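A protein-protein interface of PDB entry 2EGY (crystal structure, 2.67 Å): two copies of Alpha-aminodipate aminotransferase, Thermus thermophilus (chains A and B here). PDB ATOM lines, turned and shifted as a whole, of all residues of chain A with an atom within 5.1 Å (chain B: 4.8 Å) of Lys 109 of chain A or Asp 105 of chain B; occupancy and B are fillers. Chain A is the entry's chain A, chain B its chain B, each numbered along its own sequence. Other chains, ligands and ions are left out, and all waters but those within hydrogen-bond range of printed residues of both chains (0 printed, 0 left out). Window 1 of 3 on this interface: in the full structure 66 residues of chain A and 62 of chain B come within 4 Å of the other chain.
Asp 105 of chain A touches Lys 109 of chain B, and with the chains exchanged Lys 109 of chain A touches Asp 105 of chain B.
Lys 109 of chain A touches its own counterpart, Lys 109 of chain B.
The side-chain carboxylate of Asp 105 of chain A lies within salt-bridge range of the side-chain amino group of Lys 109 of chain A (3.4 Å).
The side-chain carboxylate (OD2) of Asp 105 of chain B is in salt-bridge range of the side-chain amino group (NZ) of Lys 109 of chain B (3.6 Å).
Along chain A the printed residues that touch a printed residue of chain B span positions 105 to 266.
Printed residues of chain B that touch a printed residue of chain A: Ala 14, Gln 101, Gln 102, Asp 105, Lys 109 and Ala 131.
Hydrophobic or aromatic side chains of chain B within 4 Å of the printed part of chain A: Ala 14 and Ala 131.
Among the printed residues, Asp or Glu carboxylates within 4 Å of a Lys or Arg side-chain nitrogen of the other chain: Asp 105 of chain A with Lys 109 of chain B (2.7 Å) and Lys 109 of chain A with Asp 105 of chain B (2.9 Å).
The side-chain carboxylate (OD1) of Asp 105 of chain A is in salt-bridge range of the side-chain amino group (NZ) of Lys 109 of chain B (2.7 Å).
The side-chain amino group (NZ) of Lys 109 of chain A is in salt-bridge range of the side-chain carboxylate (OD2) of Asp 105 of chain B.
The backbone carbonyl oxygen (O) of Gly 265 of chain A lies close to the side-chain amide oxygen (OE1) of Gln 101 of chain B, at 2.7 Å.
The backbone carbonyl oxygen (O) of Ala 266 of chain A lies close to the backbone NH (N) of Gln 102 of chain B (3.3 Å).
Lys 109 of chain A touches just these residues of chain B: Asp 105 (2.9 Å) and Lys 109 (3.6 Å).
Of the printed residues of chain A, Gln 101 of chain B touches Gly 265 (2.7 Å) and Ala 266 (3.7 Å).
Asp 105 of chain B touches two residues of chain A.
Gly 108 of chain B touches none of the printed residues of chain A.
Printed residues of chain A within 4 Å of Ala 131 of chain B: Gly 265.
The nearest residue of chain B that does not touch Lys 109 of chain A is Gly 13 of chain B (4.1 Å).
The nearest residue of chain A that does not touch Asp 105 of chain B is Ala 266 of chain A (4.2 Å).
The nearest printed residue of chain B that does not touch Gly 265 of chain A is Gln 102 of chain B (5.3 Å).
Lys 109 of chain A touches Lys 109 of chain B.
Val 110 of chain A touches Ala 14 of chain B (O to CB, 3.7 Å).
CB of Asp 105 of chain B touches O of Gly 265 of chain A, 3.7 Å away.
Ala 131 of chain B touches Gly 265 of chain A (CB to O, 3.96 Å).
Ala 266 of chain A touches Gln 101 of chain B.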
ATOM      1  N   ASP A 105      34.678 -29.899  -9.424  1.00  0.00           N
ATOM      2  CA  ASP A 105      33.258 -29.884  -9.093  1.00  0.00           C
ATOM      3  C   ASP A 105      33.044 -29.017  -7.855  1.00  0.00           C
ATOM      4  O   ASP A 105      32.012 -28.359  -7.707  1.00  0.00           O
ATOM      5  CB  ASP A 105      32.769 -31.309  -8.830  1.00  0.00           C
ATOM      6  CG  ASP A 105      31.351 -31.345  -8.313  1.00  0.00           C
ATOM      7  OD1 ASP A 105      30.454 -30.881  -9.043  1.00  0.00           O
ATOM      8  OD2 ASP A 105      31.137 -31.833  -7.179  1.00  0.00           O
ATOM      9  N   LEU A 106      34.036 -29.021  -6.971  1.00  0.00           N
ATOM     10  CA  LEU A 106      33.971 -28.248  -5.742  1.00  0.00           C
ATOM     11  C   LEU A 106      34.213 -26.772  -6.026  1.00  0.00           C
ATOM     12  O   LEU A 106      33.646 -25.907  -5.356  1.00  0.00           O
ATOM     13  CB  LEU A 106      35.000 -28.766  -4.737  1.00  0.00           C
ATOM     14  CG  LEU A 106      34.846 -30.232  -4.326  1.00  0.00           C
ATOM     15  CD1 LEU A 106      35.893 -30.580  -3.306  1.00  0.00           C
ATOM     16  CD2 LEU A 106      33.460 -30.465  -3.755  1.00  0.00           C
ATOM     17  N   VAL A 107      35.051 -26.485  -7.024  1.00  0.00           N
ATOM     18  CA  VAL A 107      35.336 -25.107  -7.393  1.00  0.00           C
ATOM     19  C   VAL A 107      34.141 -24.521  -8.115  1.00  0.00           C
ATOM     20  O   VAL A 107      33.744 -23.391  -7.849  1.00  0.00           O
ATOM     21  CB  VAL A 107      36.566 -25.008  -8.288  1.00  0.00           C
ATOM     22  CG1 VAL A 107      36.613 -23.642  -8.957  1.00  0.00           C
ATOM     23  CG2 VAL A 107      37.810 -25.205  -7.449  1.00  0.00           C
ATOM     24  N   GLY A 108      33.563 -25.282  -9.034  1.00  0.00           N
ATOM     25  CA  GLY A 108      32.395 -24.787  -9.735  1.00  0.00           C
ATOM     26  C   GLY A 108      31.316 -24.422  -8.728  1.00  0.00           C
ATOM     27  O   GLY A 108      30.729 -23.349  -8.802  1.00  0.00           O
ATOM     28  N   LYS A 109      31.074 -25.321  -7.776  1.00  0.00           N
ATOM     29  CA  LYS A 109      30.071 -25.135  -6.729  1.00  0.00           C
ATOM     30  C   LYS A 109      30.349 -23.957  -5.800  1.00  0.00           C
ATOM     31  O   LYS A 109      29.430 -23.451  -5.146  1.00  0.00           O
ATOM     32  CB  LYS A 109      29.984 -26.374  -5.834  1.00  0.00           C
ATOM     33  CG  LYS A 109      29.463 -27.646  -6.457  1.00  0.00           C
ATOM     34  CD  LYS A 109      29.518 -28.759  -5.406  1.00  0.00           C
ATOM     35  CE  LYS A 109      28.833 -30.035  -5.858  1.00  0.00           C
ATOM     36  NZ  LYS A 109      28.863 -31.062  -4.770  1.00  0.00           N
ATOM     37  N   VAL A 110      31.604 -23.527  -5.726  1.00  0.00           N
ATOM     38  CA  VAL A 110      31.958 -22.452  -4.807  1.00  0.00           C
ATOM     39  C   VAL A 110      32.138 -21.048  -5.388  1.00  0.00           C
ATOM     40  O   VAL A 110      31.985 -20.053  -4.662  1.00  0.00           O
ATOM     41  CB  VAL A 110      33.226 -22.844  -4.003  1.00  0.00           C
ATOM     42  CG1 VAL A 110      33.673 -21.703  -3.113  1.00  0.00           C
ATOM     43  CG2 VAL A 110      32.925 -24.065  -3.150  1.00  0.00           C
ATOM     44  N   PHE A 111      32.438 -20.960  -6.681  1.00  0.00           N
ATOM     45  CA  PHE A 111      32.658 -19.666  -7.323  1.00  0.00           C
ATOM     46  C   PHE A 111      31.658 -19.323  -8.422  1.00  0.00           C
ATOM     47  O   PHE A 111      31.635 -18.183  -8.872  1.00  0.00           O
ATOM     48  CB  PHE A 111      34.059 -19.611  -7.954  1.00  0.00           C
ATOM     49  CG  PHE A 111      35.187 -19.800  -6.985  1.00  0.00           C
ATOM     50  CD1 PHE A 111      35.586 -18.767  -6.151  1.00  0.00           C
ATOM     51  CD2 PHE A 111      35.862 -21.011  -6.924  1.00  0.00           C
ATOM     52  CE1 PHE A 111      36.650 -18.927  -5.265  1.00  0.00           C
ATOM     53  CE2 PHE A 111      36.926 -21.191  -6.044  1.00  0.00           C
ATOM     54  CZ  PHE A 111      37.323 -20.141  -5.209  1.00  0.00           C
ATOM     55  N   LEU A 112      30.847 -20.288  -8.857  1.00  0.00           N
ATOM     56  CA  LEU A 112      29.905 -20.058  -9.953  1.00  0.00           C
ATOM     57  C   LEU A 112      28.410 -20.091  -9.649  1.00  0.00           C
ATOM     58  O   LEU A 112      27.937 -20.950  -8.910  1.00  0.00           O
ATOM     59  CB  LEU A 112      30.167 -21.063 -11.074  1.00  0.00           C
ATOM     60  CG  LEU A 112      31.559 -21.080 -11.696  1.00  0.00           C
ATOM     61  CD1 LEU A 112      31.561 -21.929 -12.966  1.00  0.00           C
ATOM     62  CD2 LEU A 112      31.969 -19.655 -11.995  1.00  0.00           C
ATOM     63  N   GLN A 135      26.805 -25.611 -13.569  1.00  0.00           N
ATOM     64  CA  GLN A 135      26.446 -24.398 -12.841  1.00  0.00           C
ATOM     65  C   GLN A 135      25.676 -23.362 -13.650  1.00  0.00           C
ATOM     66  O   GLN A 135      25.042 -22.473 -13.085  1.00  0.00           O
ATOM     67  CB  GLN A 135      27.703 -23.750 -12.261  1.00  0.00           C
ATOM     68  CG  GLN A 135      28.376 -24.587 -11.197  1.00  0.00           C
ATOM     69  CD  GLN A 135      27.480 -24.831  -9.995  1.00  0.00           C
ATOM     70  OE1 GLN A 135      27.829 -25.587  -9.088  1.00  0.00           O
ATOM     71  NE2 GLN A 135      26.322 -24.182  -9.977  1.00  0.00           N
ATOM     72  N   ALA A 262      32.316 -27.901   0.969  1.00  0.00           N
ATOM     73  CA  ALA A 262      31.626 -28.336  -0.228  1.00  0.00           C
ATOM     74  C   ALA A 262      31.827 -29.849  -0.412  1.00  0.00           C
ATOM     75  O   ALA A 262      30.898 -30.563  -0.797  1.00  0.00           O
ATOM     76  CB  ALA A 262      32.151 -27.567  -1.438  1.00  0.00           C
ATOM     77  N   GLY A 265      29.543 -32.336   1.585  1.00  0.00           N
ATOM     78  CA  GLY A 265      28.230 -32.527   1.010  1.00  0.00           C
ATOM     79  C   GLY A 265      28.317 -33.377  -0.237  1.00  0.00           C
ATOM     80  O   GLY A 265      27.303 -33.859  -0.734  1.00  0.00           O
ATOM     81  N   ALA A 266      29.541 -33.569  -0.728  1.00  0.00           N
ATOM     82  CA  ALA A 266      29.798 -34.343  -1.943  1.00  0.00           C
ATOM     83  C   ALA A 266      29.894 -35.860  -1.754  1.00  0.00           C
ATOM     84  O   ALA A 266      29.194 -36.608  -2.437  1.00  0.00           O
ATOM     85  CB  ALA A 266      31.066 -33.827  -2.618  1.00  0.00           C
ATOM     86  N   GLY B  13      26.303 -20.331  -3.738  1.00  0.00           N
ATOM     87  CA  GLY B  13      26.424 -21.624  -3.090  1.00  0.00           C
ATOM     88  C   GLY B  13      27.427 -21.658  -1.952  1.00  0.00           C
ATOM     89  O   GLY B  13      27.307 -22.471  -1.034  1.00  0.00           O
ATOM     90  N   ALA B  14      28.421 -20.778  -1.998  1.00  0.00           N
ATOM     91  CA  ALA B  14      29.431 -20.751  -0.949  1.00  0.00           C
ATOM     92  C   ALA B  14      28.798 -20.482   0.409  1.00  0.00           C
ATOM     93  O   ALA B  14      29.267 -20.980   1.435  1.00  0.00           O
ATOM     94  CB  ALA B  14      30.467 -19.694  -1.255  1.00  0.00           C
ATOM     95  N   GLN B 101      25.875 -40.276   0.206  1.00  0.00           N
ATOM     96  CA  GLN B 101      26.082 -38.842   0.297  1.00  0.00           C
ATOM     97  C   GLN B 101      26.229 -38.272  -1.102  1.00  0.00           C
ATOM     98  O   GLN B 101      25.691 -37.212  -1.405  1.00  0.00           O
ATOM     99  CB  GLN B 101      27.335 -38.534   1.105  1.00  0.00           C
ATOM    100  CG  GLN B 101      27.624 -37.061   1.196  1.00  0.00           C
ATOM    101  CD  GLN B 101      26.443 -36.296   1.719  1.00  0.00           C
ATOM    102  OE1 GLN B 101      26.250 -35.131   1.376  1.00  0.00           O
ATOM    103  NE2 GLN B 101      25.643 -36.940   2.561  1.00  0.00           N
ATOM    104  N   GLN B 102      26.961 -38.966  -1.965  1.00  0.00           N
ATOM    105  CA  GLN B 102      27.111 -38.487  -3.334  1.00  0.00           C
ATOM    106  C   GLN B 102      25.763 -38.594  -4.057  1.00  0.00           C
ATOM    107  O   GLN B 102      25.308 -37.633  -4.675  1.00  0.00           O
ATOM    108  CB  GLN B 102      28.158 -39.300  -4.096  1.00  0.00           C
ATOM    109  CG  GLN B 102      28.470 -38.744  -5.476  1.00  0.00           C
ATOM    110  CD  GLN B 102      29.299 -39.690  -6.320  1.00  0.00           C
ATOM    111  OE1 GLN B 102      28.849 -40.780  -6.666  1.00  0.00           O
ATOM    112  NE2 GLN B 102      30.520 -39.280  -6.655  1.00  0.00           N
ATOM    113  N   ALA B 103      25.121 -39.759  -3.980  1.00  0.00           N
ATOM    114  CA  ALA B 103      23.829 -39.938  -4.642  1.00  0.00           C
ATOM    115  C   ALA B 103      22.897 -38.809  -4.238  1.00  0.00           C
ATOM    116  O   ALA B 103      22.134 -38.304  -5.054  1.00  0.00           O
ATOM    117  CB  ALA B 103      23.217 -41.282  -4.267  1.00  0.00           C
ATOM    118  N   LEU B 104      22.958 -38.413  -2.970  1.00  0.00           N
ATOM    119  CA  LEU B 104      22.113 -37.330  -2.489  1.00  0.00           C
ATOM    120  C   LEU B 104      22.469 -36.068  -3.268  1.00  0.00           C
ATOM    121  O   LEU B 104      21.591 -35.375  -3.792  1.00  0.00           O
ATOM    122  CB  LEU B 104      22.315 -37.125  -0.986  1.00  0.00           C
ATOM    123  CG  LEU B 104      21.709 -38.227  -0.106  1.00  0.00           C
ATOM    124  CD1 LEU B 104      22.043 -37.996   1.378  1.00  0.00           C
ATOM    125  CD2 LEU B 104      20.200 -38.252  -0.325  1.00  0.00           C
ATOM    126  N   ASP B 105      23.769 -35.796  -3.357  1.00  0.00           N
ATOM    127  CA  ASP B 105      24.279 -34.641  -4.078  1.00  0.00           C
ATOM    128  C   ASP B 105      23.802 -34.696  -5.526  1.00  0.00           C
ATOM    129  O   ASP B 105      23.281 -33.715  -6.048  1.00  0.00           O
ATOM    130  CB  ASP B 105      25.814 -34.631  -4.007  1.00  0.00           C
ATOM    131  CG  ASP B 105      26.433 -33.351  -4.562  1.00  0.00           C
ATOM    132  OD1 ASP B 105      26.001 -32.242  -4.160  1.00  0.00           O
ATOM    133  OD2 ASP B 105      27.369 -33.465  -5.392  1.00  0.00           O
ATOM    134  N   LEU B 106      23.967 -35.845  -6.172  1.00  0.00           N
ATOM    135  CA  LEU B 106      23.538 -35.995  -7.561  1.00  0.00           C
ATOM    136  C   LEU B 106      22.063 -35.657  -7.661  1.00  0.00           C
ATOM    137  O   LEU B 106      21.660 -34.821  -8.470  1.00  0.00           O
ATOM    138  CB  LEU B 106      23.752 -37.431  -8.059  1.00  0.00           C
ATOM    139  CG  LEU B 106      25.160 -38.032  -8.054  1.00  0.00           C
ATOM    140  CD1 LEU B 106      25.090 -39.394  -8.686  1.00  0.00           C
ATOM    141  CD2 LEU B 106      26.141 -37.146  -8.812  1.00  0.00           C
ATOM    142  N   VAL B 107      21.263 -36.323  -6.836  1.00  0.00           N
ATOM    143  CA  VAL B 107      19.821 -36.116  -6.800  1.00  0.00           C
ATOM    144  C   VAL B 107      19.490 -34.631  -6.752  1.00  0.00           C
ATOM    145  O   VAL B 107      18.631 -34.165  -7.494  1.00  0.00           O
ATOM    146  CB  VAL B 107      19.203 -36.849  -5.584  1.00  0.00           C
ATOM    147  CG1 VAL B 107      17.949 -36.131  -5.110  1.00  0.00           C
ATOM    148  CG2 VAL B 107      18.880 -38.307  -5.969  1.00  0.00           C
ATOM    149  N   GLY B 108      20.183 -33.889  -5.891  1.00  0.00           N
ATOM    150  CA  GLY B 108      19.952 -32.454  -5.781  1.00  0.00           C
ATOM    151  C   GLY B 108      20.332 -31.681  -7.039  1.00  0.00           C
ATOM    152  O   GLY B 108      19.625 -30.759  -7.453  1.00  0.00           O
ATOM    153  N   LYS B 109      21.454 -32.056  -7.647  1.00  0.00           N
ATOM    154  CA  LYS B 109      21.928 -31.413  -8.861  1.00  0.00           C
ATOM    155  C   LYS B 109      20.942 -31.544 -10.025  1.00  0.00           C
ATOM    156  O   LYS B 109      20.702 -30.576 -10.751  1.00  0.00           O
ATOM    157  CB  LYS B 109      23.264 -32.013  -9.304  1.00  0.00           C
ATOM    158  CG  LYS B 109      24.426 -31.824  -8.357  1.00  0.00           C
ATOM    159  CD  LYS B 109      25.718 -32.391  -8.971  1.00  0.00           C
ATOM    160  CE  LYS B 109      26.962 -32.052  -8.135  1.00  0.00           C
ATOM    161  NZ  LYS B 109      28.261 -32.474  -8.757  1.00  0.00           N
ATOM    162  N   ALA B 131      23.506 -31.542   1.284  1.00  0.00           N
ATOM    163  CA  ALA B 131      23.567 -31.678  -0.169  1.00  0.00           C
ATOM    164  C   ALA B 131      22.504 -30.838  -0.867  1.00  0.00           C
ATOM    165  O   ALA B 131      22.807 -30.083  -1.792  1.00  0.00           O
ATOM    166  CB  ALA B 131      23.410 -33.148  -0.574  1.00  0.00           C
ATOM    167  N   LEU B 134      22.697 -26.909  -0.858  1.00  0.00           N
ATOM    168  CA  LEU B 134      23.656 -26.408  -1.847  1.00  0.00           C
ATOM    169  C   LEU B 134      22.954 -25.892  -3.099  1.00  0.00           C
ATOM    170  O   LEU B 134      23.520 -25.125  -3.871  1.00  0.00           O
ATOM    171  CB  LEU B 134      24.630 -27.535  -2.220  1.00  0.00           C
ATOM    172  CG  LEU B 134      25.768 -27.342  -3.232  1.00  0.00           C
ATOM    173  CD1 LEU B 134      25.220 -27.389  -4.645  1.00  0.00           C
ATOM    174  CD2 LEU B 134      26.492 -26.031  -2.956  1.00  0.00           C
